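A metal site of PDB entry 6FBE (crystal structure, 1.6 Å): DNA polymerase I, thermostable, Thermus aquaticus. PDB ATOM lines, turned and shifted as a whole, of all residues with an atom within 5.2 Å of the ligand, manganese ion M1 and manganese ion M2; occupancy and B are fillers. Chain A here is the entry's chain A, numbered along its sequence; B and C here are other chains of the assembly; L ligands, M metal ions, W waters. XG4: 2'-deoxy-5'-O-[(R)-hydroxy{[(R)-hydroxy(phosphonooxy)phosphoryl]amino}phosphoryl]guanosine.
An oxygen (O1G) of the ligand lies within hydrogen-bond range of the backbone NH (N) of Gln 322 (3.0 Å).
An oxygen (O2B) of the ligand sits at hydrogen-bond distance from a ring nitrogen (NE2) of His 348 (3.0 Å).
NH2 of Arg 282 lies within hydrogen-bond range of O4' of the ligand (3.1 Å).
An oxygen (O1B) of the ligand lies close to the backbone NH (N) of Ile 323, 3.3 Å away.
O3' of the ligand sits at hydrogen-bond distance from N of Glu 324, 3.2 Å away.
NH1 of Arg 368 lies within salt-bridge range of O2G of the ligand (2.5 Å).
N3 of DG 5 of chain C sits close to a nitrogen (N2) of the ligand, at 3.3 Å.
A nitrogen (N2) of the ligand sits at hydrogen-bond distance from O2 of DC 4 of chain C (2.7 Å).
The side-chain amino group of Lys 372 lies within hydrogen-bond range of a nitrogen (N7) of the ligand (3.0 Å).
The side-chain amide nitrogen (NE2) of Gln 322 lies within hydrogen-bond range of the side-chain hydroxyl (OG) of Ser 321.
The side-chain amino group of Lys 540 lies close to the side-chain carboxylate of Asp 319, 3.8 Å away.
The side-chain carboxylate (OE1) of Glu 324 sits at hydrogen-bond distance from the side-chain hydroxyl (OH) of Tyr 380.
The guanidinium group of Arg 282 is in hydrogen-bond range of O2 of DC 12 of chain B, at 2.8 Å.
Merely in contact with the ligand: Phe 376 (3.1 Å), Tyr 380 (3.3 Å) and Ser 321 (3.4 Å).
Hydrophobic or aromatic side chains within 4 Å of the ligand: Ile 323, His 348, Phe 376 and Tyr 380.
16 residues have an atom within 4 Å of the ligand: Arg 282, Asp 319, Tyr 320, Ser 321, Gln 322, Ile 323, Glu 324, His 348, Arg 368, Lys 372, Phe 376, Tyr 380, Asp 494, DC 12 of chain B, DC 4 of chain C and DG 5 of chain C.
The nearest printed residue that does not touch the ligand is Thr 373 (4.3 Å).
Three residues have an atom within 4 Å of manganese ion M1: Asp 319, Tyr 320 and Asp 494.
The nearest printed residue that does not touch manganese ion M1 is Ser 321 (4.3 Å).
Manganese ion M1 is bound by OD2 of Asp 494.
The backbone carbonyl oxygen (O) of Tyr 320 is bound to manganese ion M1.
O3G of the ligand is bound to manganese ion M1 (2.1 Å).
The side-chain carboxylate (OD1) of Asp 319 is bound to manganese ion M1, at 2.1 Å.
Manganese ion M1 is bound by an oxygen (O1B) of the ligand, at 2.2 Å.
O1A of the ligand binds manganese ion M1, at 2.3 Å.
Manganese ion M2 is bound by OD1 of Asp 494 (2.1 Å), OD2 of Asp 319 (2.2 Å), water W2 (2.2 Å), water W1 (2.2 Å), O3' of DC 12 of chain B (2.2 Å) and O1A of the ligand (2.3 Å).
Water W2 lies within hydrogen-bond range of the side-chain carboxylate (OE1) of Glu 495 and the backbone carbonyl oxygen (O) of Val 492.
Water W8 lies within hydrogen-bond range of NZ of Lys 372 (2.6 Å), O2A of the ligand (2.7 Å) and OP2 of DC 12 of chain B (3.1 Å).
Water W5 lies within hydrogen-bond range of the side-chain amino group (NZ) of Lys 372 (2.8 Å), an oxygen (O6) of the ligand (2.8 Å), the side-chain hydroxyl (OG1) of Thr 373 (2.9 Å) and N4 of DC 12 of chain B (3.4 Å).
Water W6 lies within hydrogen-bond range of OE2 of Glu 324 (2.8 Å), NH2 of Arg 282 (3.0 Å) and O4' of the ligand (3.5 Å).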
ATOM      1  N   ARG A 282      28.874  -5.518   4.513  1.00  0.00           N
ATOM      2  CA  ARG A 282      27.486  -5.966   4.501  1.00  0.00           C
ATOM      3  C   ARG A 282      26.956  -5.995   3.075  1.00  0.00           C
ATOM      4  O   ARG A 282      27.438  -5.261   2.192  1.00  0.00           O
ATOM      5  CB  ARG A 282      26.610  -5.042   5.334  1.00  0.00           C
ATOM      6  CG  ARG A 282      26.597  -5.326   6.811  1.00  0.00           C
ATOM      7  CD  ARG A 282      25.513  -4.492   7.449  1.00  0.00           C
ATOM      8  NE  ARG A 282      25.249  -4.860   8.830  1.00  0.00           N
ATOM      9  CZ  ARG A 282      24.278  -4.324   9.562  1.00  0.00           C
ATOM     10  NH1 ARG A 282      23.480  -3.410   9.031  1.00  0.00           N
ATOM     11  NH2 ARG A 282      24.101  -4.711  10.814  1.00  0.00           N
ATOM     12  N   ASP A 319      18.558 -16.371  13.282  1.00  0.00           N
ATOM     13  CA  ASP A 319      19.130 -15.073  13.605  1.00  0.00           C
ATOM     14  C   ASP A 319      20.201 -15.210  14.680  1.00  0.00           C
ATOM     15  O   ASP A 319      19.937 -15.800  15.733  1.00  0.00           O
ATOM     16  CB  ASP A 319      18.026 -14.106  14.053  1.00  0.00           C
ATOM     17  CG  ASP A 319      18.539 -12.708  14.267  1.00  0.00           C
ATOM     18  OD1 ASP A 319      19.413 -12.539  15.137  1.00  0.00           O
ATOM     19  OD2 ASP A 319      18.095 -11.788  13.544  1.00  0.00           O
ATOM     20  N   TYR A 320      21.396 -14.688  14.405  1.00  0.00           N
ATOM     21  CA  TYR A 320      22.488 -14.770  15.376  1.00  0.00           C
ATOM     22  C   TYR A 320      22.161 -13.944  16.622  1.00  0.00           C
ATOM     23  O   TYR A 320      21.728 -12.789  16.532  1.00  0.00           O
ATOM     24  CB  TYR A 320      23.791 -14.263  14.779  1.00  0.00           C
ATOM     25  CG  TYR A 320      24.530 -15.214  13.853  1.00  0.00           C
ATOM     26  CD1 TYR A 320      25.247 -16.300  14.349  1.00  0.00           C
ATOM     27  CD2 TYR A 320      24.558 -14.983  12.482  1.00  0.00           C
ATOM     28  CE1 TYR A 320      25.935 -17.143  13.501  1.00  0.00           C
ATOM     29  CE2 TYR A 320      25.246 -15.825  11.633  1.00  0.00           C
ATOM     30  CZ  TYR A 320      25.937 -16.895  12.148  1.00  0.00           C
ATOM     31  OH  TYR A 320      26.625 -17.727  11.300  1.00  0.00           O
ATOM     32  N   SER A 321      22.423 -14.536  17.788  1.00  0.00           N
ATOM     33  CA  SER A 321      22.219 -13.858  19.062  1.00  0.00           C
ATOM     34  C   SER A 321      23.316 -12.821  19.311  1.00  0.00           C
ATOM     35  O   SER A 321      24.504 -13.156  19.267  1.00  0.00           O
ATOM     36  CB  SER A 321      22.190 -14.888  20.200  1.00  0.00           C
ATOM     37  OG  SER A 321      22.301 -14.270  21.469  1.00  0.00           O
ATOM     38  N   GLN A 322      22.918 -11.586  19.575  1.00  0.00           N
ATOM     39  CA  GLN A 322      23.823 -10.531  20.069  1.00  0.00           C
ATOM     40  C   GLN A 322      25.140 -10.515  19.291  1.00  0.00           C
ATOM     41  O   GLN A 322      26.229 -10.447  19.858  1.00  0.00           O
ATOM     42  CB  GLN A 322      24.110 -10.726  21.550  1.00  0.00           C
ATOM     43  CG  GLN A 322      22.892 -10.998  22.409  1.00  0.00           C
ATOM     44  CD  GLN A 322      23.260 -11.322  23.839  1.00  0.00           C
ATOM     45  OE1 GLN A 322      23.741 -10.465  24.579  1.00  0.00           O
ATOM     46  NE2 GLN A 322      23.051 -12.575  24.229  1.00  0.00           N
ATOM     47  N   ILE A 323      25.038 -10.559  17.956  1.00  0.00           N
ATOM     48  CA  ILE A 323      26.199 -10.996  17.171  1.00  0.00           C
ATOM     49  C   ILE A 323      27.364 -10.024  17.322  1.00  0.00           C
ATOM     50  O   ILE A 323      28.507 -10.443  17.528  1.00  0.00           O
ATOM     51  CB  ILE A 323      25.809 -11.223  15.697  1.00  0.00           C
ATOM     52  CG1 ILE A 323      27.001 -11.780  14.916  1.00  0.00           C
ATOM     53  CG2 ILE A 323      25.317  -9.940  15.036  1.00  0.00           C
ATOM     54  CD1 ILE A 323      27.633 -13.044  15.501  1.00  0.00           C
ATOM     55  N   GLU A 324      27.111  -8.714  17.213  1.00  0.00           N
ATOM     56  CA  GLU A 324      28.251  -7.797  17.220  1.00  0.00           C
ATOM     57  C   GLU A 324      28.886  -7.715  18.596  1.00  0.00           C
ATOM     58  O   GLU A 324      30.099  -7.461  18.704  1.00  0.00           O
ATOM     59  CB  GLU A 324      27.837  -6.424  16.683  1.00  0.00           C
ATOM     60  CG  GLU A 324      27.829  -6.407  15.150  1.00  0.00           C
ATOM     61  CD  GLU A 324      27.628  -5.032  14.535  1.00  0.00           C
ATOM     62  OE1 GLU A 324      27.861  -4.011  15.222  1.00  0.00           O
ATOM     63  OE2 GLU A 324      27.220  -4.973  13.360  1.00  0.00           O
ATOM     64  N   LEU A 325      28.128  -7.953  19.662  1.00  0.00           N
ATOM     65  CA  LEU A 325      28.743  -8.028  20.989  1.00  0.00           C
ATOM     66  C   LEU A 325      29.622  -9.270  21.105  1.00  0.00           C
ATOM     67  O   LEU A 325      30.672  -9.224  21.756  1.00  0.00           O
ATOM     68  CB  LEU A 325      27.680  -8.006  22.083  1.00  0.00           C
ATOM     69  CG  LEU A 325      26.804  -6.750  22.181  1.00  0.00           C
ATOM     70  CD1 LEU A 325      25.782  -6.871  23.308  1.00  0.00           C
ATOM     71  CD2 LEU A 325      27.656  -5.502  22.390  1.00  0.00           C
ATOM     72  N   HIS A 348      21.332  -7.567  26.065  1.00  0.00           N
ATOM     73  CA  HIS A 348      20.168  -6.767  25.702  1.00  0.00           C
ATOM     74  C   HIS A 348      19.091  -6.865  26.784  1.00  0.00           C
ATOM     75  O   HIS A 348      18.537  -5.854  27.225  1.00  0.00           O
ATOM     76  CB  HIS A 348      19.607  -7.210  24.345  1.00  0.00           C
ATOM     77  CG  HIS A 348      20.547  -6.981  23.208  1.00  0.00           C
ATOM     78  ND1 HIS A 348      21.491  -5.984  23.206  1.00  0.00           N
ATOM     79  CD2 HIS A 348      20.681  -7.624  22.018  1.00  0.00           C
ATOM     80  CE1 HIS A 348      22.172  -6.024  22.071  1.00  0.00           C
ATOM     81  NE2 HIS A 348      21.702  -7.013  21.337  1.00  0.00           N
ATOM     82  N   ARG A 368      13.331  -5.138  24.777  1.00  0.00           N
ATOM     83  CA  ARG A 368      14.629  -5.652  24.360  1.00  0.00           C
ATOM     84  C   ARG A 368      15.133  -4.913  23.118  1.00  0.00           C
ATOM     85  O   ARG A 368      16.321  -4.624  23.007  1.00  0.00           O
ATOM     86  CB  ARG A 368      14.540  -7.162  24.113  1.00  0.00           C
ATOM     87  CG  ARG A 368      15.896  -7.856  24.123  1.00  0.00           C
ATOM     88  CD  ARG A 368      15.765  -9.373  24.165  1.00  0.00           C
ATOM     89  NE  ARG A 368      17.067 -10.028  23.986  1.00  0.00           N
ATOM     90  CZ  ARG A 368      17.679 -10.159  22.816  1.00  0.00           C
ATOM     91  NH1 ARG A 368      17.111  -9.684  21.706  1.00  0.00           N
ATOM     92  NH2 ARG A 368      18.860 -10.753  22.743  1.00  0.00           N
ATOM     93  N   LYS A 372      18.535  -2.930  22.828  1.00  0.00           N
ATOM     94  CA  LYS A 372      19.509  -3.174  21.772  1.00  0.00           C
ATOM     95  C   LYS A 372      20.084  -1.854  21.259  1.00  0.00           C
ATOM     96  O   LYS A 372      21.303  -1.692  21.130  1.00  0.00           O
ATOM     97  CB  LYS A 372      18.867  -3.973  20.640  1.00  0.00           C
ATOM     98  CG  LYS A 372      19.768  -4.223  19.429  1.00  0.00           C
ATOM     99  CD  LYS A 372      18.973  -4.163  18.134  1.00  0.00           C
ATOM    100  CE  LYS A 372      18.574  -2.741  17.781  1.00  0.00           C
ATOM    101  NZ  LYS A 372      18.037  -2.624  16.396  1.00  0.00           N
ATOM    102  N   THR A 373      19.199  -0.885  20.981  1.00  0.00           N
ATOM    103  CA  THR A 373      19.643   0.405  20.479  1.00  0.00           C
ATOM    104  C   THR A 373      20.558   1.096  21.473  1.00  0.00           C
ATOM    105  O   THR A 373      21.573   1.702  21.083  1.00  0.00           O
ATOM    106  CB  THR A 373      18.420   1.276  20.172  1.00  0.00           C
ATOM    107  OG1 THR A 373      17.537   0.561  19.299  1.00  0.00           O
ATOM    108  CG2 THR A 373      18.836   2.576  19.498  1.00  0.00           C
ATOM    109  N   PHE A 376      24.170  -0.749  21.552  1.00  0.00           N
ATOM    110  CA  PHE A 376      25.028  -0.445  20.415  1.00  0.00           C
ATOM    111  C   PHE A 376      25.269   1.058  20.300  1.00  0.00           C
ATOM    112  O   PHE A 376      26.383   1.473  19.949  1.00  0.00           O
ATOM    113  CB  PHE A 376      24.431  -1.022  19.141  1.00  0.00           C
ATOM    114  CG  PHE A 376      24.451  -2.522  19.123  1.00  0.00           C
ATOM    115  CD1 PHE A 376      25.632  -3.201  19.330  1.00  0.00           C
ATOM    116  CD2 PHE A 376      23.275  -3.250  18.951  1.00  0.00           C
ATOM    117  CE1 PHE A 376      25.655  -4.585  19.344  1.00  0.00           C
ATOM    118  CE2 PHE A 376      23.303  -4.624  18.974  1.00  0.00           C
ATOM    119  CZ  PHE A 376      24.494  -5.290  19.163  1.00  0.00           C
ATOM    120  N   GLY A 377      24.267   1.866  20.609  1.00  0.00           N
ATOM    121  CA  GLY A 377      24.478   3.309  20.640  1.00  0.00           C
ATOM    122  C   GLY A 377      25.633   3.693  21.549  1.00  0.00           C
ATOM    123  O   GLY A 377      26.520   4.442  21.158  1.00  0.00           O
ATOM    124  N   TYR A 380      29.226   2.454  20.211  1.00  0.00           N
ATOM    125  CA  TYR A 380      29.808   3.107  19.054  1.00  0.00           C
ATOM    126  C   TYR A 380      29.857   4.629  19.185  1.00  0.00           C
ATOM    127  O   TYR A 380      29.997   5.325  18.186  1.00  0.00           O
ATOM    128  CB  TYR A 380      29.067   2.672  17.790  1.00  0.00           C
ATOM    129  CG  TYR A 380      29.248   1.184  17.502  1.00  0.00           C
ATOM    130  CD1 TYR A 380      30.510   0.643  17.286  1.00  0.00           C
ATOM    131  CD2 TYR A 380      28.152   0.311  17.481  1.00  0.00           C
ATOM    132  CE1 TYR A 380      30.679  -0.708  17.029  1.00  0.00           C
ATOM    133  CE2 TYR A 380      28.322  -1.049  17.222  1.00  0.00           C
ATOM    134  CZ  TYR A 380      29.585  -1.549  16.997  1.00  0.00           C
ATOM    135  OH  TYR A 380      29.776  -2.899  16.738  1.00  0.00           O
ATOM    136  N   ASN A 459      33.821   1.070  14.252  1.00  0.00           N
ATOM    137  CA  ASN A 459      32.641   0.248  14.015  1.00  0.00           C
ATOM    138  C   ASN A 459      32.905  -0.816  12.956  1.00  0.00           C
ATOM    139  O   ASN A 459      32.425  -1.951  13.077  1.00  0.00           O
ATOM    140  CB  ASN A 459      31.459   1.117  13.585  1.00  0.00           C
ATOM    141  CG  ASN A 459      30.270   0.306  13.093  1.00  0.00           C
ATOM    142  OD1 ASN A 459      30.168  -0.008  11.903  1.00  0.00           O
ATOM    143  ND2 ASN A 459      29.376  -0.054  14.010  1.00  0.00           N
ATOM    144  N   VAL A 492      19.107 -10.958   6.074  1.00  0.00           N
ATOM    145  CA  VAL A 492      18.904  -9.642   6.684  1.00  0.00           C
ATOM    146  C   VAL A 492      20.030  -9.413   7.682  1.00  0.00           C
ATOM    147  O   VAL A 492      19.794  -9.263   8.885  1.00  0.00           O
ATOM    148  CB  VAL A 492      17.516  -9.536   7.339  1.00  0.00           C
ATOM    149  CG1 VAL A 492      17.209  -8.083   7.682  1.00  0.00           C
ATOM    150  CG2 VAL A 492      16.430 -10.085   6.408  1.00  0.00           C
ATOM    151  N   ASP A 494      22.252 -10.478   9.822  1.00  0.00           N
ATOM    152  CA  ASP A 494      22.638 -11.588  10.674  1.00  0.00           C
ATOM    153  C   ASP A 494      21.519 -12.626  10.750  1.00  0.00           C
ATOM    154  O   ASP A 494      21.439 -13.376  11.718  1.00  0.00           O
ATOM    155  CB  ASP A 494      23.014 -11.101  12.071  1.00  0.00           C
ATOM    156  CG  ASP A 494      21.807 -10.796  12.923  1.00  0.00           C
ATOM    157  OD1 ASP A 494      20.784 -10.337  12.370  1.00  0.00           O
ATOM    158  OD2 ASP A 494      21.898 -11.012  14.147  1.00  0.00           O
ATOM    159  N   GLU A 495      20.665 -12.645   9.737  1.00  0.00           N
ATOM    160  CA  GLU A 495      19.481 -13.483   9.716  1.00  0.00           C
ATOM    161  C   GLU A 495      19.337 -14.099   8.338  1.00  0.00           C
ATOM    162  O   GLU A 495      19.640 -13.451   7.324  1.00  0.00           O
ATOM    163  CB  GLU A 495      18.230 -12.664  10.067  1.00  0.00           C
ATOM    164  CG  GLU A 495      16.901 -13.388   9.863  1.00  0.00           C
ATOM    165  CD  GLU A 495      15.717 -12.461  10.024  1.00  0.00           C
ATOM    166  OE1 GLU A 495      15.921 -11.279  10.361  1.00  0.00           O
ATOM    167  OE2 GLU A 495      14.576 -12.910   9.817  1.00  0.00           O
ATOM    168  N   LYS A 540       9.762 -16.159  13.373  1.00  0.00           N
ATOM    169  CA  LYS A 540      10.662 -15.537  14.347  1.00  0.00           C
ATOM    170  C   LYS A 540      10.140 -15.664  15.771  1.00  0.00           C
ATOM    171  O   LYS A 540      10.473 -14.840  16.627  1.00  0.00           O
ATOM    172  CB  LYS A 540      10.900 -14.066  13.993  1.00  0.00           C
ATOM    173  CG  LYS A 540      11.391 -13.839  12.561  1.00  0.00           C
ATOM    174  CD  LYS A 540      12.198 -12.553  12.445  1.00  0.00           C
ATOM    175  CE  LYS A 540      13.627 -12.746  12.926  1.00  0.00           C
ATOM    176  NZ  LYS A 540      14.359 -11.458  13.085  1.00  0.00           N
ATOM    177  P    DC B  12      14.827  -5.739  12.208  1.00  0.00           P
ATOM    178  OP1  DC B  12      14.350  -7.138  12.257  1.00  0.00           O
ATOM    179  OP2  DC B  12      14.614  -4.833  13.351  1.00  0.00           O
ATOM    180  O5'  DC B  12      16.389  -5.725  11.892  1.00  0.00           O
ATOM    181  C5'  DC B  12      16.921  -6.600  10.903  1.00  0.00           C
ATOM    182  C4'  DC B  12      18.414  -6.397  10.743  1.00  0.00           C
ATOM    183  O4'  DC B  12      18.657  -5.025  10.378  1.00  0.00           O
ATOM    184  C3'  DC B  12      19.235  -6.613  12.009  1.00  0.00           C
ATOM    185  O3'  DC B  12      19.652  -7.972  12.104  1.00  0.00           O
ATOM    186  C2'  DC B  12      20.414  -5.671  11.839  1.00  0.00           C
ATOM    187  C1'  DC B  12      19.886  -4.580  10.910  1.00  0.00           C
ATOM    188  N1   DC B  12      19.678  -3.283  11.582  1.00  0.00           N
ATOM    189  C2   DC B  12      20.732  -2.379  11.656  1.00  0.00           C
ATOM    190  O2   DC B  12      21.821  -2.706  11.176  1.00  0.00           O
ATOM    191  N3   DC B  12      20.520  -1.180  12.227  1.00  0.00           N
ATOM    192  C4   DC B  12      19.318  -0.872  12.730  1.00  0.00           C
ATOM    193  N4   DC B  12      19.165   0.330  13.299  1.00  0.00           N
ATOM    194  C5   DC B  12      18.226  -1.780  12.669  1.00  0.00           C
ATOM    195  C6   DC B  12      18.439  -2.967  12.086  1.00  0.00           C
ATOM    196  P    DC C   4      25.255  11.024  19.037  1.00  0.00           P
ATOM    197  OP1  DC C   4      23.930  11.163  18.389  1.00  0.00           O
ATOM    198  OP2  DC C   4      25.421  11.395  20.452  1.00  0.00           O
ATOM    199  O5'  DC C   4      25.688   9.499  18.857  1.00  0.00           O
ATOM    200  C5'  DC C   4      25.699   8.922  17.561  1.00  0.00           C
ATOM    201  C4'  DC C   4      26.546   7.676  17.531  1.00  0.00           C
ATOM    202  O4'  DC C   4      25.950   6.666  18.381  1.00  0.00           O
ATOM    203  C3'  DC C   4      26.676   7.014  16.163  1.00  0.00           C
ATOM    204  O3'  DC C   4      27.748   7.586  15.422  1.00  0.00           O
ATOM    205  C2'  DC C   4      26.935   5.562  16.532  1.00  0.00           C
ATOM    206  C1'  DC C   4      26.078   5.386  17.774  1.00  0.00           C
ATOM    207  N1   DC C   4      24.715   4.851  17.500  1.00  0.00           N
ATOM    208  C2   DC C   4      24.564   3.520  17.082  1.00  0.00           C
ATOM    209  O2   DC C   4      25.576   2.822  16.943  1.00  0.00           O
ATOM    210  N3   DC C   4      23.328   3.038  16.850  1.00  0.00           N
ATOM    211  C4   DC C   4      22.263   3.830  17.019  1.00  0.00           C
ATOM    212  N4   DC C   4      21.054   3.311  16.766  1.00  0.00           N
ATOM    213  C5   DC C   4      22.390   5.188  17.443  1.00  0.00           C
ATOM    214  C6   DC C   4      23.622   5.651  17.664  1.00  0.00           C
ATOM    215  P    DG C   5      27.588   7.881  13.844  1.00  0.00           P
ATOM    216  OP1  DG C   5      28.704   8.793  13.473  1.00  0.00           O
ATOM    217  OP2  DG C   5      26.191   8.292  13.575  1.00  0.00           O
ATOM    218  O5'  DG C   5      27.810   6.454  13.164  1.00  0.00           O
ATOM    219  C5'  DG C   5      29.055   5.801  13.272  1.00  0.00           C
ATOM    220  C4'  DG C   5      28.947   4.354  12.840  1.00  0.00           C
ATOM    221  O4'  DG C   5      28.038   3.655  13.715  1.00  0.00           O
ATOM    222  C3'  DG C   5      28.380   4.137  11.446  1.00  0.00           C
ATOM    223  O3'  DG C   5      29.380   4.282  10.442  1.00  0.00           O
ATOM    224  C2'  DG C   5      27.842   2.719  11.544  1.00  0.00           C
ATOM    225  C1'  DG C   5      27.349   2.651  12.991  1.00  0.00           C
ATOM    226  N9   DG C   5      25.913   2.869  13.125  1.00  0.00           N
ATOM    227  C8   DG C   5      25.272   4.004  13.586  1.00  0.00           C
ATOM    228  N7   DG C   5      23.969   3.892  13.594  1.00  0.00           N
ATOM    229  C5   DG C   5      23.748   2.593  13.128  1.00  0.00           C
ATOM    230  C6   DG C   5      22.545   1.879  12.915  1.00  0.00           C
ATOM    231  O6   DG C   5      21.379   2.247  13.114  1.00  0.00           O
ATOM    232  N1   DG C   5      22.793   0.592  12.421  1.00  0.00           N
ATOM    233  C2   DG C   5      24.041   0.075  12.169  1.00  0.00           C
ATOM    234  N2   DG C   5      24.094  -1.166  11.697  1.00  0.00           N
ATOM    235  N3   DG C   5      25.156   0.736  12.363  1.00  0.00           N
ATOM    236  C4   DG C   5      24.945   1.977  12.829  1.00  0.00           C
HETATM  237  N1  XG4 L   1      23.155   0.433  15.946  1.00  0.00           N
HETATM  238  C2  XG4 L   1      24.286  -0.211  15.519  1.00  0.00           C
HETATM  239  N2  XG4 L   1      25.431   0.464  15.612  1.00  0.00           N
HETATM  240  N3  XG4 L   1      24.295  -1.456  15.052  1.00  0.00           N
HETATM  241  C4  XG4 L   1      23.081  -2.026  15.061  1.00  0.00           C
HETATM  242  C5  XG4 L   1      21.886  -1.473  15.461  1.00  0.00           C
HETATM  243  C6  XG4 L   1      21.882  -0.131  15.957  1.00  0.00           C
HETATM  244  O6  XG4 L   1      20.918   0.504  16.382  1.00  0.00           O
HETATM  245  N7  XG4 L   1      20.854  -2.398  15.323  1.00  0.00           N
HETATM  246  C8  XG4 L   1      21.442  -3.477  14.865  1.00  0.00           C
HETATM  247  N9  XG4 L   1      22.799  -3.323  14.706  1.00  0.00           N
HETATM  248  PA  XG4 L   1      19.890  -7.711  15.600  1.00  0.00           P
HETATM  249  PB  XG4 L   1      21.414  -8.660  17.926  1.00  0.00           P
HETATM  250  PG  XG4 L   1      19.489 -10.512  19.051  1.00  0.00           P
HETATM  251  C1' XG4 L   1      23.805  -4.355  14.411  1.00  0.00           C
HETATM  252  O1A XG4 L   1      19.790  -9.077  15.085  1.00  0.00           O
HETATM  253  O1B XG4 L   1      22.022  -9.609  17.001  1.00  0.00           O
HETATM  254  O1G XG4 L   1      19.986 -11.537  20.077  1.00  0.00           O
HETATM  255  C2' XG4 L   1      24.415  -4.937  15.676  1.00  0.00           C
HETATM  256  O2A XG4 L   1      18.494  -7.017  15.414  1.00  0.00           O
HETATM  257  O2B XG4 L   1      22.541  -7.790  18.559  1.00  0.00           O
HETATM  258  O2G XG4 L   1      18.152  -9.922  19.403  1.00  0.00           O
HETATM  259  C3' XG4 L   1      23.580  -6.188  15.908  1.00  0.00           C
HETATM  260  O3' XG4 L   1      24.335  -7.150  16.641  1.00  0.00           O
HETATM  261  N3A XG4 L   1      20.348  -7.682  17.156  1.00  0.00           N
HETATM  262  O3B XG4 L   1      20.593  -9.359  19.090  1.00  0.00           O
HETATM  263  O3G XG4 L   1      19.525 -11.090  17.607  1.00  0.00           O
HETATM  264  C4' XG4 L   1      23.333  -6.643  14.478  1.00  0.00           C
HETATM  265  O4' XG4 L   1      23.161  -5.420  13.725  1.00  0.00           O
HETATM  266  C5' XG4 L   1      22.141  -7.550  14.278  1.00  0.00           C
HETATM  267  O5' XG4 L   1      20.955  -6.899  14.789  1.00  0.00           O
HETATM  268 MN    MN M   1      20.740 -11.055  15.883  1.00  0.00          MN
HETATM  269 MN    MN M   2      18.844  -9.819  13.093  1.00  0.00          MN
HETATM  270  O   HOH W   1      17.052  -8.836  13.962  1.00  0.00           O
HETATM  271  O   HOH W   2      17.672  -9.838  11.259  1.00  0.00           O
HETATM  272  O   HOH W   3      16.860 -10.518  16.465  1.00  0.00           O
HETATM  273  O   HOH W   4      18.730 -13.971  17.655  1.00  0.00           O
HETATM  274  O   HOH W   5      18.133   0.160  16.541  1.00  0.00           O
HETATM  275  O   HOH W   6      25.771  -6.934  11.997  1.00  0.00           O
HETATM  276  O   HOH W   7      18.483 -13.707  20.557  1.00  0.00           O
HETATM  277  O   HOH W   8      17.079  -4.711  15.159  1.00  0.00           O
HETATM  278  O   HOH W   9      17.767  -7.213  18.850  1.00  0.00           O
HETATM  279  O   HOH W  10      26.915  -1.855  13.625  1.00  0.00           O
